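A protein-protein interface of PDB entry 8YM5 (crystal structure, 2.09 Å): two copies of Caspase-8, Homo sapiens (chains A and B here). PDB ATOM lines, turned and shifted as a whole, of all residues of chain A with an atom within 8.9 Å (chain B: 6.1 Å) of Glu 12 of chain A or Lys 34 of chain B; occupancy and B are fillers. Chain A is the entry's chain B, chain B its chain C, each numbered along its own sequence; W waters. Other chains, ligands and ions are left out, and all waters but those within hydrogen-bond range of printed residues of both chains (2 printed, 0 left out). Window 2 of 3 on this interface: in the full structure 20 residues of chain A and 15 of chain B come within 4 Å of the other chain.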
ATOM      1  N   ARG A   5     -28.929 -19.737   4.141  1.00  0.00           N
ATOM      2  CA  ARG A   5     -27.727 -18.979   4.427  1.00  0.00           C
ATOM      3  C   ARG A   5     -27.927 -18.057   5.625  1.00  0.00           C
ATOM      4  O   ARG A   5     -27.043 -17.937   6.478  1.00  0.00           O
ATOM      5  CB  ARG A   5     -27.317 -18.176   3.203  1.00  0.00           C
ATOM      6  CG  ARG A   5     -25.974 -17.479   3.379  1.00  0.00           C
ATOM      7  CD  ARG A   5     -25.574 -16.770   2.103  1.00  0.00           C
ATOM      8  NE  ARG A   5     -24.313 -16.052   2.244  1.00  0.00           N
ATOM      9  CZ  ARG A   5     -23.776 -15.305   1.288  1.00  0.00           C
ATOM     10  NH1 ARG A   5     -24.362 -15.166   0.108  1.00  0.00           N
ATOM     11  NH2 ARG A   5     -22.637 -14.659   1.533  1.00  0.00           N
ATOM     12  N   ASN A   6     -29.090 -17.403   5.703  1.00  0.00           N
ATOM     13  CA  ASN A   6     -29.373 -16.502   6.814  1.00  0.00           C
ATOM     14  C   ASN A   6     -29.417 -17.253   8.139  1.00  0.00           C
ATOM     15  O   ASN A   6     -28.888 -16.769   9.148  1.00  0.00           O
ATOM     16  CB  ASN A   6     -30.712 -15.777   6.576  1.00  0.00           C
ATOM     17  CG  ASN A   6     -30.755 -14.421   7.234  1.00  0.00           C
ATOM     18  OD1 ASN A   6     -29.778 -13.682   7.176  1.00  0.00           O
ATOM     19  ND2 ASN A   6     -31.893 -14.076   7.859  1.00  0.00           N
ATOM     20  N   LEU A   7     -30.076 -18.421   8.165  1.00  0.00           N
ATOM     21  CA  LEU A   7     -30.078 -19.244   9.379  1.00  0.00           C
ATOM     22  C   LEU A   7     -28.662 -19.659   9.762  1.00  0.00           C
ATOM     23  O   LEU A   7     -28.295 -19.649  10.950  1.00  0.00           O
ATOM     24  CB  LEU A   7     -30.940 -20.506   9.182  1.00  0.00           C
ATOM     25  CG  LEU A   7     -32.463 -20.340   9.091  1.00  0.00           C
ATOM     26  CD1 LEU A   7     -33.159 -21.700   9.029  1.00  0.00           C
ATOM     27  CD2 LEU A   7     -33.015 -19.501  10.254  1.00  0.00           C
ATOM     28  N   TYR A   8     -27.859 -20.051   8.770  1.00  0.00           N
ATOM     29  CA  TYR A   8     -26.479 -20.425   9.050  1.00  0.00           C
ATOM     30  C   TYR A   8     -25.711 -19.263   9.677  1.00  0.00           C
ATOM     31  O   TYR A   8     -24.983 -19.458  10.658  1.00  0.00           O
ATOM     32  CB  TYR A   8     -25.798 -20.932   7.765  1.00  0.00           C
ATOM     33  CG  TYR A   8     -24.297 -21.032   7.914  1.00  0.00           C
ATOM     34  CD1 TYR A   8     -23.715 -22.084   8.604  1.00  0.00           C
ATOM     35  CD2 TYR A   8     -23.469 -20.052   7.394  1.00  0.00           C
ATOM     36  CE1 TYR A   8     -22.333 -22.163   8.762  1.00  0.00           C
ATOM     37  CE2 TYR A   8     -22.080 -20.127   7.539  1.00  0.00           C
ATOM     38  CZ  TYR A   8     -21.529 -21.169   8.229  1.00  0.00           C
ATOM     39  OH  TYR A   8     -20.167 -21.222   8.363  1.00  0.00           O
ATOM     40  N   ASP A   9     -25.873 -18.041   9.137  1.00  0.00           N
ATOM     41  CA  ASP A   9     -25.136 -16.883   9.662  1.00  0.00           C
ATOM     42  C   ASP A   9     -25.543 -16.586  11.103  1.00  0.00           C
ATOM     43  O   ASP A   9     -24.698 -16.325  11.992  1.00  0.00           O
ATOM     44  CB  ASP A   9     -25.393 -15.652   8.777  1.00  0.00           C
ATOM     45  CG  ASP A   9     -24.771 -15.780   7.377  1.00  0.00           C
ATOM     46  OD1 ASP A   9     -23.796 -16.532   7.219  1.00  0.00           O
ATOM     47  OD2 ASP A   9     -25.216 -15.094   6.430  1.00  0.00           O
ATOM     48  N   ILE A  10     -26.852 -16.622  11.352  1.00  0.00           N
ATOM     49  CA  ILE A  10     -27.363 -16.431  12.707  1.00  0.00           C
ATOM     50  C   ILE A  10     -26.720 -17.430  13.649  1.00  0.00           C
ATOM     51  O   ILE A  10     -26.252 -17.079  14.747  1.00  0.00           O
ATOM     52  CB  ILE A  10     -28.896 -16.559  12.721  1.00  0.00           C
ATOM     53  CG1 ILE A  10     -29.523 -15.351  12.037  1.00  0.00           C
ATOM     54  CG2 ILE A  10     -29.383 -16.750  14.147  1.00  0.00           C
ATOM     55  CD1 ILE A  10     -31.100 -15.446  11.845  1.00  0.00           C
ATOM     56  N   GLY A  11     -26.682 -18.694  13.225  1.00  0.00           N
ATOM     57  CA  GLY A  11     -26.097 -19.737  14.047  1.00  0.00           C
ATOM     58  C   GLY A  11     -24.621 -19.523  14.306  1.00  0.00           C
ATOM     59  O   GLY A  11     -24.111 -19.899  15.363  1.00  0.00           O
ATOM     60  N   GLU A  12     -23.904 -18.952  13.336  1.00  0.00           N
ATOM     61  CA  GLU A  12     -22.482 -18.713  13.565  1.00  0.00           C
ATOM     62  C   GLU A  12     -22.263 -17.654  14.629  1.00  0.00           C
ATOM     63  O   GLU A  12     -21.160 -17.576  15.181  1.00  0.00           O
ATOM     64  CB  GLU A  12     -21.771 -18.297  12.271  1.00  0.00           C
ATOM     65  CG  GLU A  12     -21.574 -19.446  11.302  1.00  0.00           C
ATOM     66  CD  GLU A  12     -20.775 -20.598  11.911  1.00  0.00           C
ATOM     67  OE1 GLU A  12     -19.521 -20.496  11.992  1.00  0.00           O
ATOM     68  OE2 GLU A  12     -21.412 -21.593  12.329  1.00  0.00           O
ATOM     69  N   GLN A  13     -23.266 -16.812  14.905  1.00  0.00           N
ATOM     70  CA  GLN A  13     -23.107 -15.808  15.961  1.00  0.00           C
ATOM     71  C   GLN A  13     -23.596 -16.257  17.350  1.00  0.00           C
ATOM     72  O   GLN A  13     -23.627 -15.435  18.275  1.00  0.00           O
ATOM     73  CB  GLN A  13     -23.801 -14.501  15.553  1.00  0.00           C
ATOM     74  CG  GLN A  13     -23.100 -13.769  14.370  1.00  0.00           C
ATOM     75  CD  GLN A  13     -21.734 -13.124  14.726  1.00  0.00           C
ATOM     76  OE1 GLN A  13     -21.235 -13.227  15.852  1.00  0.00           O
ATOM     77  NE2 GLN A  13     -21.139 -12.437  13.749  1.00  0.00           N
ATOM     78  N   LEU A  14     -23.981 -17.518  17.523  1.00  0.00           N
ATOM     79  CA  LEU A  14     -24.509 -18.023  18.789  1.00  0.00           C
ATOM     80  C   LEU A  14     -23.542 -19.059  19.356  1.00  0.00           C
ATOM     81  O   LEU A  14     -23.299 -20.093  18.723  1.00  0.00           O
ATOM     82  CB  LEU A  14     -25.891 -18.666  18.582  1.00  0.00           C
ATOM     83  CG  LEU A  14     -27.040 -17.753  18.168  1.00  0.00           C
ATOM     84  CD1 LEU A  14     -28.261 -18.560  17.599  1.00  0.00           C
ATOM     85  CD2 LEU A  14     -27.458 -16.863  19.358  1.00  0.00           C
ATOM     86  N   ASP A  15     -23.010 -18.806  20.551  1.00  0.00           N
ATOM     87  CA  ASP A  15     -22.061 -19.744  21.141  1.00  0.00           C
ATOM     88  C   ASP A  15     -22.809 -20.705  22.074  1.00  0.00           C
ATOM     89  O   ASP A  15     -24.044 -20.758  22.093  1.00  0.00           O
ATOM     90  CB  ASP A  15     -20.903 -18.986  21.793  1.00  0.00           C
ATOM     91  CG  ASP A  15     -21.316 -18.120  22.986  1.00  0.00           C
ATOM     92  OD1 ASP A  15     -22.329 -18.386  23.680  1.00  0.00           O
ATOM     93  OD2 ASP A  15     -20.592 -17.134  23.224  1.00  0.00           O
ATOM     94  N   SER A  16     -22.066 -21.489  22.855  1.00  0.00           N
ATOM     95  CA  SER A  16     -22.690 -22.569  23.614  1.00  0.00           C
ATOM     96  C   SER A  16     -23.550 -22.060  24.773  1.00  0.00           C
ATOM     97  O   SER A  16     -24.504 -22.738  25.161  1.00  0.00           O
ATOM     98  CB  SER A  16     -21.614 -23.546  24.116  1.00  0.00           C
ATOM     99  OG  SER A  16     -20.844 -22.962  25.132  1.00  0.00           O
ATOM    100  N   ASP A  18     -25.336 -19.034  24.739  1.00  0.00           N
ATOM    101  CA  ASP A  18     -26.564 -18.609  24.059  1.00  0.00           C
ATOM    102  C   ASP A  18     -27.409 -19.819  23.687  1.00  0.00           C
ATOM    103  O   ASP A  18     -28.640 -19.801  23.812  1.00  0.00           O
ATOM    104  CB  ASP A  18     -26.219 -17.762  22.824  1.00  0.00           C
ATOM    105  CG  ASP A  18     -25.947 -16.294  23.189  1.00  0.00           C
ATOM    106  OD1 ASP A  18     -25.932 -16.004  24.399  1.00  0.00           O
ATOM    107  OD2 ASP A  18     -25.711 -15.437  22.296  1.00  0.00           O
ATOM    108  N   ASP A  40     -25.468 -27.296  18.455  1.00  0.00           N
ATOM    109  CA  ASP A  40     -25.282 -26.004  17.809  1.00  0.00           C
ATOM    110  C   ASP A  40     -26.655 -25.492  17.398  1.00  0.00           C
ATOM    111  O   ASP A  40     -27.647 -26.226  17.446  1.00  0.00           O
ATOM    112  CB  ASP A  40     -24.325 -26.091  16.621  1.00  0.00           C
ATOM    113  CG  ASP A  40     -24.932 -26.823  15.434  1.00  0.00           C
ATOM    114  OD1 ASP A  40     -25.162 -28.040  15.541  1.00  0.00           O
ATOM    115  OD2 ASP A  40     -25.203 -26.169  14.402  1.00  0.00           O
ATOM    116  N   ALA A  41     -26.717 -24.204  17.035  1.00  0.00           N
ATOM    117  CA  ALA A  41     -28.010 -23.589  16.753  1.00  0.00           C
ATOM    118  C   ALA A  41     -28.700 -24.220  15.547  1.00  0.00           C
ATOM    119  O   ALA A  41     -29.928 -24.279  15.513  1.00  0.00           O
ATOM    120  CB  ALA A  41     -27.853 -22.076  16.551  1.00  0.00           C
ATOM    121  N   LEU A  42     -27.943 -24.697  14.553  1.00  0.00           N
ATOM    122  CA  LEU A  42     -28.574 -25.265  13.364  1.00  0.00           C
ATOM    123  C   LEU A  42     -29.394 -26.511  13.685  1.00  0.00           C
ATOM    124  O   LEU A  42     -30.421 -26.760  13.039  1.00  0.00           O
ATOM    125  CB  LEU A  42     -27.520 -25.595  12.305  1.00  0.00           C
ATOM    126  CG  LEU A  42     -27.045 -24.402  11.486  1.00  0.00           C
ATOM    127  CD1 LEU A  42     -26.399 -24.893  10.219  1.00  0.00           C
ATOM    128  CD2 LEU A  42     -28.193 -23.467  11.178  1.00  0.00           C
ATOM    129  N   PHE A  45     -32.580 -25.236  15.085  1.00  0.00           N
ATOM    130  CA  PHE A  45     -33.449 -24.738  14.014  1.00  0.00           C
ATOM    131  C   PHE A  45     -34.083 -25.881  13.229  1.00  0.00           C
ATOM    132  O   PHE A  45     -35.246 -25.787  12.821  1.00  0.00           O
ATOM    133  CB  PHE A  45     -32.672 -23.840  13.045  1.00  0.00           C
ATOM    134  CG  PHE A  45     -32.083 -22.600  13.673  1.00  0.00           C
ATOM    135  CD1 PHE A  45     -32.518 -22.145  14.908  1.00  0.00           C
ATOM    136  CD2 PHE A  45     -31.075 -21.902  13.019  1.00  0.00           C
ATOM    137  CE1 PHE A  45     -31.957 -21.020  15.491  1.00  0.00           C
ATOM    138  CE2 PHE A  45     -30.505 -20.774  13.598  1.00  0.00           C
ATOM    139  CZ  PHE A  45     -30.964 -20.323  14.829  1.00  0.00           C
ATOM    140  N   ARG A  71     -30.412 -10.839  22.198  1.00  0.00           N
ATOM    141  CA  ARG A  71     -29.594 -10.732  20.990  1.00  0.00           C
ATOM    142  C   ARG A  71     -30.256  -9.781  19.990  1.00  0.00           C
ATOM    143  O   ARG A  71     -30.692 -10.161  18.896  1.00  0.00           O
ATOM    144  CB  ARG A  71     -29.367 -12.112  20.388  1.00  0.00           C
ATOM    145  CG  ARG A  71     -28.438 -13.044  21.227  1.00  0.00           C
ATOM    146  CD  ARG A  71     -27.113 -12.368  21.632  1.00  0.00           C
ATOM    147  NE  ARG A  71     -26.287 -12.054  20.468  1.00  0.00           N
ATOM    148  CZ  ARG A  71     -25.353 -12.861  19.975  1.00  0.00           C
ATOM    149  NH1 ARG A  71     -25.111 -14.050  20.516  1.00  0.00           N
ATOM    150  NH2 ARG A  71     -24.645 -12.466  18.918  1.00  0.00           N
ATOM    151  N   LEU A  74     -28.560  -9.443  16.541  1.00  0.00           N
ATOM    152  CA  LEU A  74     -28.939 -10.411  15.516  1.00  0.00           C
ATOM    153  C   LEU A  74     -30.312 -10.096  14.933  1.00  0.00           C
ATOM    154  O   LEU A  74     -30.532 -10.248  13.722  1.00  0.00           O
ATOM    155  CB  LEU A  74     -28.905 -11.823  16.106  1.00  0.00           C
ATOM    156  CG  LEU A  74     -27.532 -12.311  16.613  1.00  0.00           C
ATOM    157  CD1 LEU A  74     -27.632 -13.748  17.086  1.00  0.00           C
ATOM    158  CD2 LEU A  74     -26.463 -12.165  15.549  1.00  0.00           C
ATOM    159  N   TYR A  78     -29.852  -9.556  10.999  1.00  0.00           N
ATOM    160  CA  TYR A  78     -30.280 -10.635  10.133  1.00  0.00           C
ATOM    161  C   TYR A  78     -31.787 -10.762   9.990  1.00  0.00           C
ATOM    162  O   TYR A  78     -32.238 -11.494   9.097  1.00  0.00           O
ATOM    163  CB  TYR A  78     -29.683 -11.963  10.625  1.00  0.00           C
ATOM    164  CG  TYR A  78     -28.157 -11.979  10.568  1.00  0.00           C
ATOM    165  CD1 TYR A  78     -27.497 -12.061   9.342  1.00  0.00           C
ATOM    166  CD2 TYR A  78     -27.391 -11.892  11.724  1.00  0.00           C
ATOM    167  CE1 TYR A  78     -26.104 -12.056   9.268  1.00  0.00           C
ATOM    168  CE2 TYR A  78     -25.984 -11.885  11.665  1.00  0.00           C
ATOM    169  CZ  TYR A  78     -25.357 -11.977  10.424  1.00  0.00           C
ATOM    170  OH  TYR A  78     -23.985 -11.978  10.321  1.00  0.00           O
ATOM    171  N   ILE B  30     -14.507 -12.759  12.838  1.00  0.00           N
ATOM    172  CA  ILE B  30     -14.646 -14.089  13.417  1.00  0.00           C
ATOM    173  C   ILE B  30     -15.865 -14.066  14.319  1.00  0.00           C
ATOM    174  O   ILE B  30     -15.838 -13.428  15.380  1.00  0.00           O
ATOM    175  CB  ILE B  30     -13.401 -14.513  14.215  1.00  0.00           C
ATOM    176  CG1 ILE B  30     -12.155 -14.423  13.338  1.00  0.00           C
ATOM    177  CG2 ILE B  30     -13.591 -15.956  14.718  1.00  0.00           C
ATOM    178  CD1 ILE B  30     -10.871 -14.729  14.105  1.00  0.00           C
ATOM    179  N   PRO B  31     -16.934 -14.746  13.946  1.00  0.00           N
ATOM    180  CA  PRO B  31     -18.188 -14.652  14.705  1.00  0.00           C
ATOM    181  C   PRO B  31     -18.091 -15.442  16.006  1.00  0.00           C
ATOM    182  O   PRO B  31     -17.198 -16.278  16.208  1.00  0.00           O
ATOM    183  CB  PRO B  31     -19.224 -15.263  13.738  1.00  0.00           C
ATOM    184  CG  PRO B  31     -18.421 -16.222  12.897  1.00  0.00           C
ATOM    185  CD  PRO B  31     -17.051 -15.568  12.727  1.00  0.00           C
ATOM    186  N   GLN B  32     -19.079 -15.212  16.869  1.00  0.00           N
ATOM    187  CA  GLN B  32     -18.997 -15.640  18.273  1.00  0.00           C
ATOM    188  C   GLN B  32     -18.874 -17.156  18.417  1.00  0.00           C
ATOM    189  O   GLN B  32     -18.122 -17.652  19.280  1.00  0.00           O
ATOM    190  CB  GLN B  32     -20.219 -15.125  19.044  1.00  0.00           C
ATOM    191  CG  GLN B  32     -20.136 -13.617  19.356  1.00  0.00           C
ATOM    192  CD  GLN B  32     -19.106 -13.329  20.447  1.00  0.00           C
ATOM    193  OE1 GLN B  32     -19.349 -13.583  21.623  1.00  0.00           O
ATOM    194  NE2 GLN B  32     -17.940 -12.842  20.049  1.00  0.00           N
ATOM    195  N   ARG B  33     -19.590 -17.910  17.583  1.00  0.00           N
ATOM    196  CA  ARG B  33     -19.479 -19.371  17.664  1.00  0.00           C
ATOM    197  C   ARG B  33     -18.045 -19.829  17.432  1.00  0.00           C
ATOM    198  O   ARG B  33     -17.570 -20.756  18.095  1.00  0.00           O
ATOM    199  CB  ARG B  33     -20.408 -20.060  16.660  1.00  0.00           C
ATOM    200  CG  ARG B  33     -20.461 -21.623  16.793  1.00  0.00           C
ATOM    201  CD  ARG B  33     -21.062 -22.290  15.555  1.00  0.00           C
ATOM    202  NE  ARG B  33     -21.129 -23.749  15.654  1.00  0.00           N
ATOM    203  CZ  ARG B  33     -21.191 -24.569  14.612  1.00  0.00           C
ATOM    204  NH1 ARG B  33     -21.185 -24.106  13.368  1.00  0.00           N
ATOM    205  NH2 ARG B  33     -21.262 -25.887  14.821  1.00  0.00           N
ATOM    206  N   LYS B  34     -17.353 -19.212  16.472  1.00  0.00           N
ATOM    207  CA  LYS B  34     -15.964 -19.550  16.172  1.00  0.00           C
ATOM    208  C   LYS B  34     -14.971 -18.891  17.131  1.00  0.00           C
ATOM    209  O   LYS B  34     -13.831 -19.355  17.236  1.00  0.00           O
ATOM    210  CB  LYS B  34     -15.623 -19.163  14.722  1.00  0.00           C
ATOM    211  CG  LYS B  34     -16.516 -19.867  13.645  1.00  0.00           C
ATOM    212  CD  LYS B  34     -16.030 -21.297  13.367  1.00  0.00           C
ATOM    213  CE  LYS B  34     -16.673 -21.912  12.096  1.00  0.00           C
ATOM    214  NZ  LYS B  34     -17.997 -22.547  12.401  1.00  0.00           N
ATOM    215  N   GLN B  35     -15.370 -17.831  17.828  1.00  0.00           N
ATOM    216  CA  GLN B  35     -14.505 -17.217  18.835  1.00  0.00           C
ATOM    217  C   GLN B  35     -14.357 -18.117  20.052  1.00  0.00           C
ATOM    218  O   GLN B  35     -13.268 -18.221  20.631  1.00  0.00           O
ATOM    219  CB  GLN B  35     -15.075 -15.868  19.284  1.00  0.00           C
ATOM    220  CG  GLN B  35     -15.000 -14.765  18.253  1.00  0.00           C
ATOM    221  CD  GLN B  35     -13.906 -13.775  18.558  1.00  0.00           C
ATOM    222  OE1 GLN B  35     -13.326 -13.797  19.653  1.00  0.00           O
ATOM    223  NE2 GLN B  35     -13.587 -12.918  17.586  1.00  0.00           N
ATOM    224  N   GLU B  36     -15.450 -18.762  20.466  1.00  0.00           N
ATOM    225  CA  GLU B  36     -15.436 -19.468  21.746  1.00  0.00           C
ATOM    226  C   GLU B  36     -14.287 -20.469  21.919  1.00  0.00           C
ATOM    227  O   GLU B  36     -13.627 -20.434  22.966  1.00  0.00           O
ATOM    228  CB  GLU B  36     -16.787 -20.166  21.944  1.00  0.00           C
ATOM    229  CG  GLU B  36     -16.918 -20.844  23.282  1.00  0.00           C
ATOM    230  CD  GLU B  36     -18.325 -21.357  23.521  1.00  0.00           C
ATOM    231  OE1 GLU B  36     -19.047 -21.595  22.528  1.00  0.00           O
ATOM    232  OE2 GLU B  36     -18.705 -21.532  24.697  1.00  0.00           O
ATOM    233  N   PRO B  37     -14.006 -21.392  20.994  1.00  0.00           N
ATOM    234  CA  PRO B  37     -12.911 -22.338  21.258  1.00  0.00           C
ATOM    235  C   PRO B  37     -11.508 -21.788  21.005  1.00  0.00           C
ATOM    236  O   PRO B  37     -10.535 -22.510  21.236  1.00  0.00           O
ATOM    237  CB  PRO B  37     -13.225 -23.499  20.304  1.00  0.00           C
ATOM    238  CG  PRO B  37     -13.903 -22.845  19.157  1.00  0.00           C
ATOM    239  CD  PRO B  37     -14.728 -21.730  19.746  1.00  0.00           C
ATOM    240  N   ILE B  38     -11.322 -20.541  20.588  1.00  0.00           N
ATOM    241  CA  ILE B  38      -9.964 -20.084  20.286  1.00  0.00           C
ATOM    242  C   ILE B  38      -9.216 -19.834  21.594  1.00  0.00           C
ATOM    243  O   ILE B  38      -9.543 -18.904  22.336  1.00  0.00           O
ATOM    244  CB  ILE B  38      -9.976 -18.835  19.409  1.00  0.00           C
ATOM    245  CG1 ILE B  38     -10.569 -19.170  18.035  1.00  0.00           C
ATOM    246  CG2 ILE B  38      -8.568 -18.273  19.298  1.00  0.00           C
ATOM    247  CD1 ILE B  38     -10.615 -17.957  17.115  1.00  0.00           C
ATOM    248  N   ARG B  47      -8.290 -19.430  11.611  1.00  0.00           N
ATOM    249  CA  ARG B  47      -9.498 -18.709  11.183  1.00  0.00           C
ATOM    250  C   ARG B  47      -9.180 -17.681  10.105  1.00  0.00           C
ATOM    251  O   ARG B  47      -9.921 -17.533   9.120  1.00  0.00           O
ATOM    252  CB  ARG B  47     -10.154 -17.924  12.344  1.00  0.00           C
ATOM    253  CG  ARG B  47     -10.802 -18.688  13.487  1.00  0.00           C
ATOM    254  CD  ARG B  47     -11.997 -19.446  13.040  1.00  0.00           C
ATOM    255  NE  ARG B  47     -11.641 -20.801  12.631  1.00  0.00           N
ATOM    256  CZ  ARG B  47     -12.384 -21.532  11.820  1.00  0.00           C
ATOM    257  NH1 ARG B  47     -13.508 -21.055  11.309  1.00  0.00           N
ATOM    258  NH2 ARG B  47     -11.994 -22.770  11.514  1.00  0.00           N
HETATM  259  O   HOH W   1     -18.938 -23.417   9.498  1.00  0.00           O
HETATM  260  O   HOH W   2     -17.984 -16.771  22.073  1.00  0.00           O
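Water W1 bridges the side-chain hydroxyl of Tyr 8 of chain A and the side-chain amino group of Lys 34 of chain B. Water W2 bridges OD2 of Asp 15 of chain A (2.9 Å) and O of Gln 32 of chain B (2.9 Å).
The backbone NH of Gln 32 of chain B sits at hydrogen-bond distance from the side-chain amide oxygen of Gln 13 of chain A, 3.1 Å away. The guanidinium group of Arg 33 of chain B lies within salt-bridge range of the side-chain carboxylate of Glu 12 of chain A (2.7 Å). The guanidinium group (NH2) of Arg 33 of chain B is in salt-bridge range of the side-chain carboxylate (OD2) of Asp 40 of chain A, at 3.97 Å. The side-chain carboxylate (OE1) of Glu 12 of chain A is in salt-bridge range of the side-chain amino group (NZ) of Lys 34 of chain B (2.6 Å). The side-chain carboxylate of Glu 36 of chain B lies within hydrogen-bond range of the side-chain hydroxyl of Ser 16 of chain A, 2.6 Å away.
Arg 33 of chain B touches Gly 11 of chain A. O of Glu 12 of chain A touches CB of Pro 31 of chain B, at 3.3 Å. Gln 32 of chain B touches Glu 12 of chain A. Gln 13 of chain A touches Pro 31 of chain B. O of Leu 14 of chain A touches CB of Arg 33 of chain B, at 3.6 Å. Gln 32 of chain B touches Asp 15 of chain A. CB of Asp 15 of chain A touches OE1 of Glu 36 of chain B, 3.3 Å away.
Of the 20 printed residues of chain A, 7 touch a printed residue of chain B. Among the printed residues, 12 pairs touch across the chains.
The guanidinium group (NH1) of Arg 71 of chain A is in hydrogen-bond range of the backbone carbonyl oxygen (O) of Gln 13 of chain A, 3.0 Å away. OD1 of Asp 15 of chain A lies within hydrogen-bond range of N of Asp 18 of chain A (3.3 Å). The side-chain carboxylate of Asp 40 of chain A lies within hydrogen-bond range of the backbone NH of Leu 42 of chain A.
No position is printed for both chains. Of the 12 pairs that touch across the chains among the printed residues, none has its exchanged pair printed and touching as well.
Of chain B, only Pro 31 (3.3 Å), Gln 32 (3.6 Å), Arg 33 (2.7 Å) and Lys 34 (2.6 Å) come within 4 Å of Glu 12 of chain A. Printed residues of chain B within 4 Å of Gln 13 of chain A: Pro 31 (3.4 Å) and Gln 32 (3.1 Å). Printed residues of chain B within 4 Å of Asp 15 of chain A: Gln 32 and Glu 36. Of the printed residues of chain B, Ser 16 of chain A touches Glu 36 (2.6 Å). Of chain A, only Glu 12 and Gln 13 come within 4 Å of Pro 31 of chain B. Of the printed residues of chain A, Arg 33 of chain B touches Gly 11, Glu 12, Leu 14 and Asp 40. Lys 34 of chain B touches just one residue of chain A: Glu 12 (2.6 Å). Printed residues of chain A within 4 Å of Glu 36 of chain B: Asp 15 (3.3 Å) and Ser 16 (2.6 Å). The nearest residue of chain A that does not touch Lys 34 of chain B is Tyr 8 of chain A (4.8 Å).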
